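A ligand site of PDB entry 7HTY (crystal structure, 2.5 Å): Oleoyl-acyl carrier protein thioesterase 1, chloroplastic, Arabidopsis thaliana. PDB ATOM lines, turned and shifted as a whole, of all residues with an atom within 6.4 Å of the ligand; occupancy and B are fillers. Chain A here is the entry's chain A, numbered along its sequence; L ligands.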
ATOM      1  N   GLY A  41     -17.446   9.758   5.325  1.00  0.00           N
ATOM      2  CA  GLY A  41     -17.544   8.400   4.790  1.00  0.00           C
ATOM      3  C   GLY A  41     -17.051   8.314   3.360  1.00  0.00           C
ATOM      4  O   GLY A  41     -16.308   7.386   3.020  1.00  0.00           O
ATOM      5  N   HIS A  44     -13.221   8.775   3.397  1.00  0.00           N
ATOM      6  CA  HIS A  44     -12.555   7.560   3.851  1.00  0.00           C
ATOM      7  C   HIS A  44     -12.434   6.577   2.669  1.00  0.00           C
ATOM      8  O   HIS A  44     -11.336   6.084   2.420  1.00  0.00           O
ATOM      9  CB  HIS A  44     -13.346   6.940   5.029  1.00  0.00           C
ATOM     10  CG  HIS A  44     -12.835   5.630   5.522  1.00  0.00           C
ATOM     11  ND1 HIS A  44     -13.602   4.824   6.343  1.00  0.00           N
ATOM     12  CD2 HIS A  44     -11.650   5.001   5.286  1.00  0.00           C
ATOM     13  CE1 HIS A  44     -12.864   3.757   6.600  1.00  0.00           C
ATOM     14  NE2 HIS A  44     -11.695   3.804   5.972  1.00  0.00           N
ATOM     15  N   ALA A  45     -13.535   6.354   1.905  1.00  0.00           N
ATOM     16  CA  ALA A  45     -13.522   5.461   0.749  1.00  0.00           C
ATOM     17  C   ALA A  45     -12.596   5.963  -0.379  1.00  0.00           C
ATOM     18  O   ALA A  45     -11.961   5.156  -1.042  1.00  0.00           O
ATOM     19  CB  ALA A  45     -14.934   5.255   0.220  1.00  0.00           C
ATOM     20  N   GLN A  46     -12.520   7.279  -0.578  1.00  0.00           N
ATOM     21  CA  GLN A  46     -11.662   7.861  -1.595  1.00  0.00           C
ATOM     22  C   GLN A  46     -10.184   7.684  -1.200  1.00  0.00           C
ATOM     23  O   GLN A  46      -9.357   7.356  -2.054  1.00  0.00           O
ATOM     24  CB  GLN A  46     -12.004   9.346  -1.808  1.00  0.00           C
ATOM     25  CG  GLN A  46     -11.454   9.959  -3.106  1.00  0.00           C
ATOM     26  CD  GLN A  46     -11.732  11.457  -3.249  1.00  0.00           C
ATOM     27  OE1 GLN A  46     -12.725  11.899  -3.873  1.00  0.00           O
ATOM     28  NE2 GLN A  46     -10.843  12.268  -2.693  1.00  0.00           N
ATOM     29  N   VAL A  48      -8.846   5.309   0.380  1.00  0.00           N
ATOM     30  CA  VAL A  48      -8.403   3.902   0.319  1.00  0.00           C
ATOM     31  C   VAL A  48      -8.556   3.284  -1.081  1.00  0.00           C
ATOM     32  O   VAL A  48      -8.566   2.062  -1.191  1.00  0.00           O
ATOM     33  CB  VAL A  48      -9.022   2.999   1.409  1.00  0.00           C
ATOM     34  CG1 VAL A  48      -8.601   3.448   2.806  1.00  0.00           C
ATOM     35  CG2 VAL A  48     -10.541   2.925   1.295  1.00  0.00           C
ATOM     36  N   PHE A  50     -11.124   3.745  -3.599  1.00  0.00           N
ATOM     37  CA  PHE A  50     -12.412   3.750  -4.289  1.00  0.00           C
ATOM     38  C   PHE A  50     -12.638   5.020  -5.119  1.00  0.00           C
ATOM     39  O   PHE A  50     -12.600   6.123  -4.591  1.00  0.00           O
ATOM     40  CB  PHE A  50     -13.575   3.454  -3.332  1.00  0.00           C
ATOM     41  CG  PHE A  50     -13.460   2.079  -2.714  1.00  0.00           C
ATOM     42  CD1 PHE A  50     -13.898   0.960  -3.394  1.00  0.00           C
ATOM     43  CD2 PHE A  50     -12.888   1.911  -1.465  1.00  0.00           C
ATOM     44  CE1 PHE A  50     -13.771  -0.299  -2.834  1.00  0.00           C
ATOM     45  CE2 PHE A  50     -12.766   0.649  -0.913  1.00  0.00           C
ATOM     46  CZ  PHE A  50     -13.220  -0.447  -1.594  1.00  0.00           C
ATOM     47  N   PHE A  55     -20.200   4.881  -4.391  1.00  0.00           N
ATOM     48  CA  PHE A  55     -19.680   4.864  -3.026  1.00  0.00           C
ATOM     49  C   PHE A  55     -19.211   3.487  -2.614  1.00  0.00           C
ATOM     50  O   PHE A  55     -20.037   2.592  -2.451  1.00  0.00           O
ATOM     51  CB  PHE A  55     -20.689   5.414  -1.991  1.00  0.00           C
ATOM     52  CG  PHE A  55     -20.252   5.286  -0.548  1.00  0.00           C
ATOM     53  CD1 PHE A  55     -19.225   6.059  -0.041  1.00  0.00           C
ATOM     54  CD2 PHE A  55     -20.873   4.383   0.303  1.00  0.00           C
ATOM     55  CE1 PHE A  55     -18.821   5.928   1.292  1.00  0.00           C
ATOM     56  CE2 PHE A  55     -20.461   4.249   1.632  1.00  0.00           C
ATOM     57  CZ  PHE A  55     -19.435   5.020   2.115  1.00  0.00           C
ATOM     58  N   ALA A  56     -17.889   3.330  -2.401  1.00  0.00           N
ATOM     59  CA  ALA A  56     -17.239   2.095  -1.964  1.00  0.00           C
ATOM     60  C   ALA A  56     -17.614   0.855  -2.783  1.00  0.00           C
ATOM     61  O   ALA A  56     -17.709  -0.229  -2.228  1.00  0.00           O
ATOM     62  CB  ALA A  56     -17.475   1.862  -0.476  1.00  0.00           C
ATOM     63  N   THR A  58     -16.538  -1.972  -5.121  1.00  0.00           N
ATOM     64  CA  THR A  58     -15.344  -2.717  -5.515  1.00  0.00           C
ATOM     65  C   THR A  58     -15.295  -2.974  -7.049  1.00  0.00           C
ATOM     66  O   THR A  58     -16.211  -2.580  -7.767  1.00  0.00           O
ATOM     67  CB  THR A  58     -15.215  -4.017  -4.667  1.00  0.00           C
ATOM     68  OG1 THR A  58     -16.035  -5.047  -5.234  1.00  0.00           O
ATOM     69  CG2 THR A  58     -15.528  -3.821  -3.169  1.00  0.00           C
ATOM     70  N   TRP A  68     -23.918  -0.410  -2.701  1.00  0.00           N
ATOM     71  CA  TRP A  68     -24.187  -0.481  -1.277  1.00  0.00           C
ATOM     72  C   TRP A  68     -25.344   0.486  -1.015  1.00  0.00           C
ATOM     73  O   TRP A  68     -25.297   1.638  -1.479  1.00  0.00           O
ATOM     74  CB  TRP A  68     -22.950  -0.009  -0.488  1.00  0.00           C
ATOM     75  CG  TRP A  68     -21.837  -1.004  -0.424  1.00  0.00           C
ATOM     76  CD1 TRP A  68     -20.565  -0.852  -0.900  1.00  0.00           C
ATOM     77  CD2 TRP A  68     -21.857  -2.269   0.268  1.00  0.00           C
ATOM     78  NE1 TRP A  68     -19.795  -1.942  -0.560  1.00  0.00           N
ATOM     79  CE2 TRP A  68     -20.571  -2.831   0.138  1.00  0.00           C
ATOM     80  CE3 TRP A  68     -22.825  -2.962   0.982  1.00  0.00           C
ATOM     81  CZ2 TRP A  68     -20.245  -4.075   0.685  1.00  0.00           C
ATOM     82  CZ3 TRP A  68     -22.509  -4.196   1.504  1.00  0.00           C
ATOM     83  CH2 TRP A  68     -21.245  -4.742   1.341  1.00  0.00           C
ATOM     84  N   TRP A  92     -15.319   4.362  10.506  1.00  0.00           N
ATOM     85  CA  TRP A  92     -14.760   3.082  10.097  1.00  0.00           C
ATOM     86  C   TRP A  92     -15.875   2.172   9.605  1.00  0.00           C
ATOM     87  O   TRP A  92     -17.044   2.389   9.931  1.00  0.00           O
ATOM     88  CB  TRP A  92     -13.985   2.429  11.252  1.00  0.00           C
ATOM     89  CG  TRP A  92     -14.823   2.026  12.439  1.00  0.00           C
ATOM     90  CD1 TRP A  92     -15.311   0.784  12.700  1.00  0.00           C
ATOM     91  CD2 TRP A  92     -15.160   2.842  13.568  1.00  0.00           C
ATOM     92  NE1 TRP A  92     -15.998   0.791  13.894  1.00  0.00           N
ATOM     93  CE2 TRP A  92     -15.904   2.045  14.449  1.00  0.00           C
ATOM     94  CE3 TRP A  92     -14.916   4.178  13.920  1.00  0.00           C
ATOM     95  CZ2 TRP A  92     -16.384   2.530  15.669  1.00  0.00           C
ATOM     96  CZ3 TRP A  92     -15.402   4.656  15.109  1.00  0.00           C
ATOM     97  CH2 TRP A  92     -16.127   3.837  15.974  1.00  0.00           C
ATOM     98  N   CYS A  93     -15.518   1.151   8.824  1.00  0.00           N
ATOM     99  CA  CYS A  93     -16.488   0.196   8.348  1.00  0.00           C
ATOM    100  C   CYS A  93     -16.154  -1.190   8.871  1.00  0.00           C
ATOM    101  O   CYS A  93     -14.991  -1.516   9.075  1.00  0.00           O
ATOM    102  CB  CYS A  93     -16.601   0.214   6.832  1.00  0.00           C
ATOM    103  SG  CYS A  93     -17.795  -0.957   6.161  1.00  0.00           S
ATOM    104  N   GLN A  94     -17.173  -1.989   9.119  1.00  0.00           N
ATOM    105  CA  GLN A  94     -16.988  -3.350   9.586  1.00  0.00           C
ATOM    106  C   GLN A  94     -17.940  -4.283   8.873  1.00  0.00           C
ATOM    107  O   GLN A  94     -19.055  -3.906   8.543  1.00  0.00           O
ATOM    108  CB  GLN A  94     -17.207  -3.459  11.090  1.00  0.00           C
ATOM    109  CG  GLN A  94     -15.980  -3.122  11.905  1.00  0.00           C
ATOM    110  CD  GLN A  94     -15.909  -4.047  13.071  1.00  0.00           C
ATOM    111  OE1 GLN A  94     -16.579  -3.851  14.073  1.00  0.00           O
ATOM    112  NE2 GLN A  94     -15.111  -5.086  12.965  1.00  0.00           N
ATOM    113  N   THR A 101     -22.763  -4.729   5.563  1.00  0.00           N
ATOM    114  CA  THR A 101     -21.767  -3.980   6.305  1.00  0.00           C
ATOM    115  C   THR A 101     -22.383  -3.011   7.308  1.00  0.00           C
ATOM    116  O   THR A 101     -23.575  -2.694   7.263  1.00  0.00           O
ATOM    117  CB  THR A 101     -20.775  -3.286   5.334  1.00  0.00           C
ATOM    118  OG1 THR A 101     -21.484  -2.625   4.302  1.00  0.00           O
ATOM    119  CG2 THR A 101     -19.816  -4.221   4.727  1.00  0.00           C
ATOM    120  N   ARG A 102     -21.547  -2.522   8.220  1.00  0.00           N
ATOM    121  CA  ARG A 102     -21.953  -1.540   9.189  1.00  0.00           C
ATOM    122  C   ARG A 102     -20.914  -0.421   9.196  1.00  0.00           C
ATOM    123  O   ARG A 102     -19.720  -0.729   9.194  1.00  0.00           O
ATOM    124  CB  ARG A 102     -22.017  -2.193  10.570  1.00  0.00           C
ATOM    125  CG  ARG A 102     -22.539  -1.258  11.644  1.00  0.00           C
ATOM    126  CD  ARG A 102     -22.351  -1.824  13.043  1.00  0.00           C
ATOM    127  NE  ARG A 102     -20.968  -1.693  13.499  1.00  0.00           N
ATOM    128  CZ  ARG A 102     -20.140  -2.713  13.669  1.00  0.00           C
ATOM    129  NH1 ARG A 102     -18.900  -2.502  14.089  1.00  0.00           N
ATOM    130  NH2 ARG A 102     -20.536  -3.956  13.440  1.00  0.00           N
ATOM    131  N   ARG A 103     -21.339   0.847   9.158  1.00  0.00           N
ATOM    132  CA  ARG A 103     -20.372   1.957   9.261  1.00  0.00           C
ATOM    133  C   ARG A 103     -20.689   2.769  10.525  1.00  0.00           C
ATOM    134  O   ARG A 103     -21.858   3.092  10.754  1.00  0.00           O
ATOM    135  CB  ARG A 103     -20.339   2.845   8.002  1.00  0.00           C
ATOM    136  CG  ARG A 103     -19.420   4.054   8.151  1.00  0.00           C
ATOM    137  CD  ARG A 103     -19.274   4.855   6.873  1.00  0.00           C
ATOM    138  NE  ARG A 103     -18.333   4.256   5.925  1.00  0.00           N
ATOM    139  CZ  ARG A 103     -17.019   4.459   5.939  1.00  0.00           C
ATOM    140  NH1 ARG A 103     -16.244   3.893   5.009  1.00  0.00           N
ATOM    141  NH2 ARG A 103     -16.462   5.212   6.878  1.00  0.00           N
ATOM    142  N   SER A 121     -24.739   2.946  11.044  1.00  0.00           N
ATOM    143  CA  SER A 121     -25.570   2.711   9.871  1.00  0.00           C
ATOM    144  C   SER A 121     -25.434   1.252   9.427  1.00  0.00           C
ATOM    145  O   SER A 121     -24.360   0.666   9.592  1.00  0.00           O
ATOM    146  CB  SER A 121     -25.158   3.641   8.726  1.00  0.00           C
ATOM    147  OG  SER A 121     -23.841   3.330   8.294  1.00  0.00           O
ATOM    148  N   TRP A 123     -25.714  -1.181   6.105  1.00  0.00           N
ATOM    149  CA  TRP A 123     -25.795  -1.189   4.648  1.00  0.00           C
ATOM    150  C   TRP A 123     -25.974  -2.586   4.096  1.00  0.00           C
ATOM    151  O   TRP A 123     -25.445  -3.537   4.651  1.00  0.00           O
ATOM    152  CB  TRP A 123     -24.521  -0.598   4.028  1.00  0.00           C
ATOM    153  CG  TRP A 123     -24.213   0.797   4.490  1.00  0.00           C
ATOM    154  CD1 TRP A 123     -23.754   1.167   5.716  1.00  0.00           C
ATOM    155  CD2 TRP A 123     -24.228   1.980   3.693  1.00  0.00           C
ATOM    156  NE1 TRP A 123     -23.568   2.529   5.749  1.00  0.00           N
ATOM    157  CE2 TRP A 123     -23.833   3.052   4.507  1.00  0.00           C
ATOM    158  CE3 TRP A 123     -24.545   2.239   2.350  1.00  0.00           C
ATOM    159  CZ2 TRP A 123     -23.753   4.363   4.041  1.00  0.00           C
ATOM    160  CZ3 TRP A 123     -24.474   3.544   1.893  1.00  0.00           C
ATOM    161  CH2 TRP A 123     -24.067   4.583   2.730  1.00  0.00           C
ATOM    162  N   GLU A 143     -12.304  -8.251  -1.270  1.00  0.00           N
ATOM    163  CA  GLU A 143     -11.981  -6.941  -1.812  1.00  0.00           C
ATOM    164  C   GLU A 143     -12.131  -5.800  -0.800  1.00  0.00           C
ATOM    165  O   GLU A 143     -11.328  -4.862  -0.851  1.00  0.00           O
ATOM    166  CB  GLU A 143     -12.794  -6.691  -3.084  1.00  0.00           C
ATOM    167  CG  GLU A 143     -12.429  -7.658  -4.191  1.00  0.00           C
ATOM    168  CD  GLU A 143     -13.322  -7.664  -5.417  1.00  0.00           C
ATOM    169  OE1 GLU A 143     -14.442  -7.120  -5.340  1.00  0.00           O
ATOM    170  OE2 GLU A 143     -12.914  -8.247  -6.454  1.00  0.00           O
ATOM    171  N   TYR A 144     -13.126  -5.856   0.111  1.00  0.00           N
ATOM    172  CA  TYR A 144     -13.321  -4.767   1.048  1.00  0.00           C
ATOM    173  C   TYR A 144     -12.907  -5.090   2.491  1.00  0.00           C
ATOM    174  O   TYR A 144     -12.711  -4.164   3.269  1.00  0.00           O
ATOM    175  CB  TYR A 144     -14.761  -4.218   0.999  1.00  0.00           C
ATOM    176  CG  TYR A 144     -15.797  -5.052   1.702  1.00  0.00           C
ATOM    177  CD1 TYR A 144     -16.007  -4.931   3.063  1.00  0.00           C
ATOM    178  CD2 TYR A 144     -16.633  -5.888   0.989  1.00  0.00           C
ATOM    179  CE1 TYR A 144     -16.949  -5.705   3.723  1.00  0.00           C
ATOM    180  CE2 TYR A 144     -17.608  -6.658   1.630  1.00  0.00           C
ATOM    181  CZ  TYR A 144     -17.761  -6.558   3.001  1.00  0.00           C
ATOM    182  OH  TYR A 144     -18.718  -7.299   3.654  1.00  0.00           O
ATOM    183  N   LEU A 145     -12.751  -6.376   2.846  1.00  0.00           N
ATOM    184  CA  LEU A 145     -12.359  -6.789   4.192  1.00  0.00           C
ATOM    185  C   LEU A 145     -11.011  -6.248   4.613  1.00  0.00           C
ATOM    186  O   LEU A 145     -10.764  -6.058   5.805  1.00  0.00           O
ATOM    187  CB  LEU A 145     -12.318  -8.305   4.298  1.00  0.00           C
ATOM    188  CG  LEU A 145     -13.592  -8.937   4.806  1.00  0.00           C
ATOM    189  CD1 LEU A 145     -13.583 -10.442   4.608  1.00  0.00           C
ATOM    190  CD2 LEU A 145     -13.844  -8.548   6.265  1.00  0.00           C
ATOM    191  N   PHE A 147      -9.897  -3.312   4.206  1.00  0.00           N
ATOM    192  CA  PHE A 147     -10.028  -1.931   4.716  1.00  0.00           C
ATOM    193  C   PHE A 147     -10.767  -1.837   6.073  1.00  0.00           C
ATOM    194  O   PHE A 147     -10.913  -0.739   6.612  1.00  0.00           O
ATOM    195  CB  PHE A 147     -10.741  -1.050   3.661  1.00  0.00           C
ATOM    196  CG  PHE A 147     -10.092  -1.136   2.308  1.00  0.00           C
ATOM    197  CD1 PHE A 147      -8.804  -0.665   2.103  1.00  0.00           C
ATOM    198  CD2 PHE A 147     -10.732  -1.765   1.255  1.00  0.00           C
ATOM    199  CE1 PHE A 147      -8.181  -0.812   0.881  1.00  0.00           C
ATOM    200  CE2 PHE A 147     -10.121  -1.887   0.014  1.00  0.00           C
ATOM    201  CZ  PHE A 147      -8.841  -1.420  -0.157  1.00  0.00           C
ATOM    202  N   CYS A 148     -11.212  -2.964   6.616  1.00  0.00           N
ATOM    203  CA  CYS A 148     -11.992  -3.044   7.828  1.00  0.00           C
ATOM    204  C   CYS A 148     -11.218  -3.682   8.949  1.00  0.00           C
ATOM    205  O   CYS A 148     -10.582  -4.710   8.724  1.00  0.00           O
ATOM    206  CB  CYS A 148     -13.286  -3.814   7.559  1.00  0.00           C
ATOM    207  SG  CYS A 148     -14.218  -3.217   6.131  1.00  0.00           S
HETATM  208  N1  LIG L   1     -18.537   0.121   2.771  1.00  0.00           N
HETATM  209  N2  LIG L   1     -17.072   1.534   3.668  1.00  0.00           N
HETATM  210  C1  LIG L   1     -14.363  -0.678   2.192  1.00  0.00           C
HETATM  211  C2  LIG L   1     -16.387   0.576   2.932  1.00  0.00           C
HETATM  212  C3  LIG L   1     -17.285  -0.276   2.363  1.00  0.00           C
HETATM  213  C4  LIG L   1     -19.807  -0.357   2.528  1.00  0.00           C
HETATM  214  C5  LIG L   1     -20.854   0.283   3.075  1.00  0.00           C
HETATM  215  C6  LIG L   1     -18.371   1.243   3.585  1.00  0.00           C
HETATM  216  C7  LIG L   1     -14.443   1.798   1.959  1.00  0.00           C
HETATM  217  C8  LIG L   1     -14.873   0.615   2.827  1.00  0.00           C
HETATM  218  C9  LIG L   1     -14.247   0.767   4.213  1.00  0.00           C
HETATM  219  C10 LIG L   1     -20.621   1.399   3.886  1.00  0.00           C
HETATM  220  N3  LIG L   1     -19.422   1.904   4.110  1.00  0.00           N
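The guanidinium group (NH1) of Arg 103 sits at hydrogen-bond distance from a nitrogen (N2) of the ligand (2.8 Å).
SG of Cys 93 lies close to N2 of the ligand.
A ring nitrogen (ND1) of His 44 lies within hydrogen-bond range of the guanidinium group (NH2) of Arg 103, 2.9 Å away.
The backbone NH of Ser 121 lies within hydrogen-bond range of the backbone carbonyl oxygen of Arg 103 (2.9 Å).
O of Thr 101 lies within hydrogen-bond range of N of Trp 123, at 2.9 Å.
SG of Cys 93 lies close to O of Arg 102 (3.6 Å).
The indole nitrogen (NE1) of Trp 68 sits at hydrogen-bond distance from the backbone carbonyl oxygen (O) of Ala 56.
The backbone NH (N) of Phe 50 is in hydrogen-bond range of the backbone carbonyl oxygen (O) of Ala 45 (3.0 Å).
NE1 of Trp 123 is in hydrogen-bond range of OG of Ser 121 (2.7 Å).
The backbone carbonyl oxygen (O) of Tyr 144 lies within hydrogen-bond range of the side-chain sulfur (SG) of Cys 148 (3.4 Å).
Residues that only touch the ligand: Thr 101, Trp 68, Phe 50, Ala 56, Phe 55, Trp 123, Tyr 144, Ala 45 and Phe 147.
Hydrophobic or aromatic side chains within 4 Å of the ligand: Ala 45, Phe 50, Phe 55, Ala 56, Trp 68, Trp 123, Tyr 144 and Phe 147.
The nearest printed residue that does not touch the ligand is His 44 (4.1 Å).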
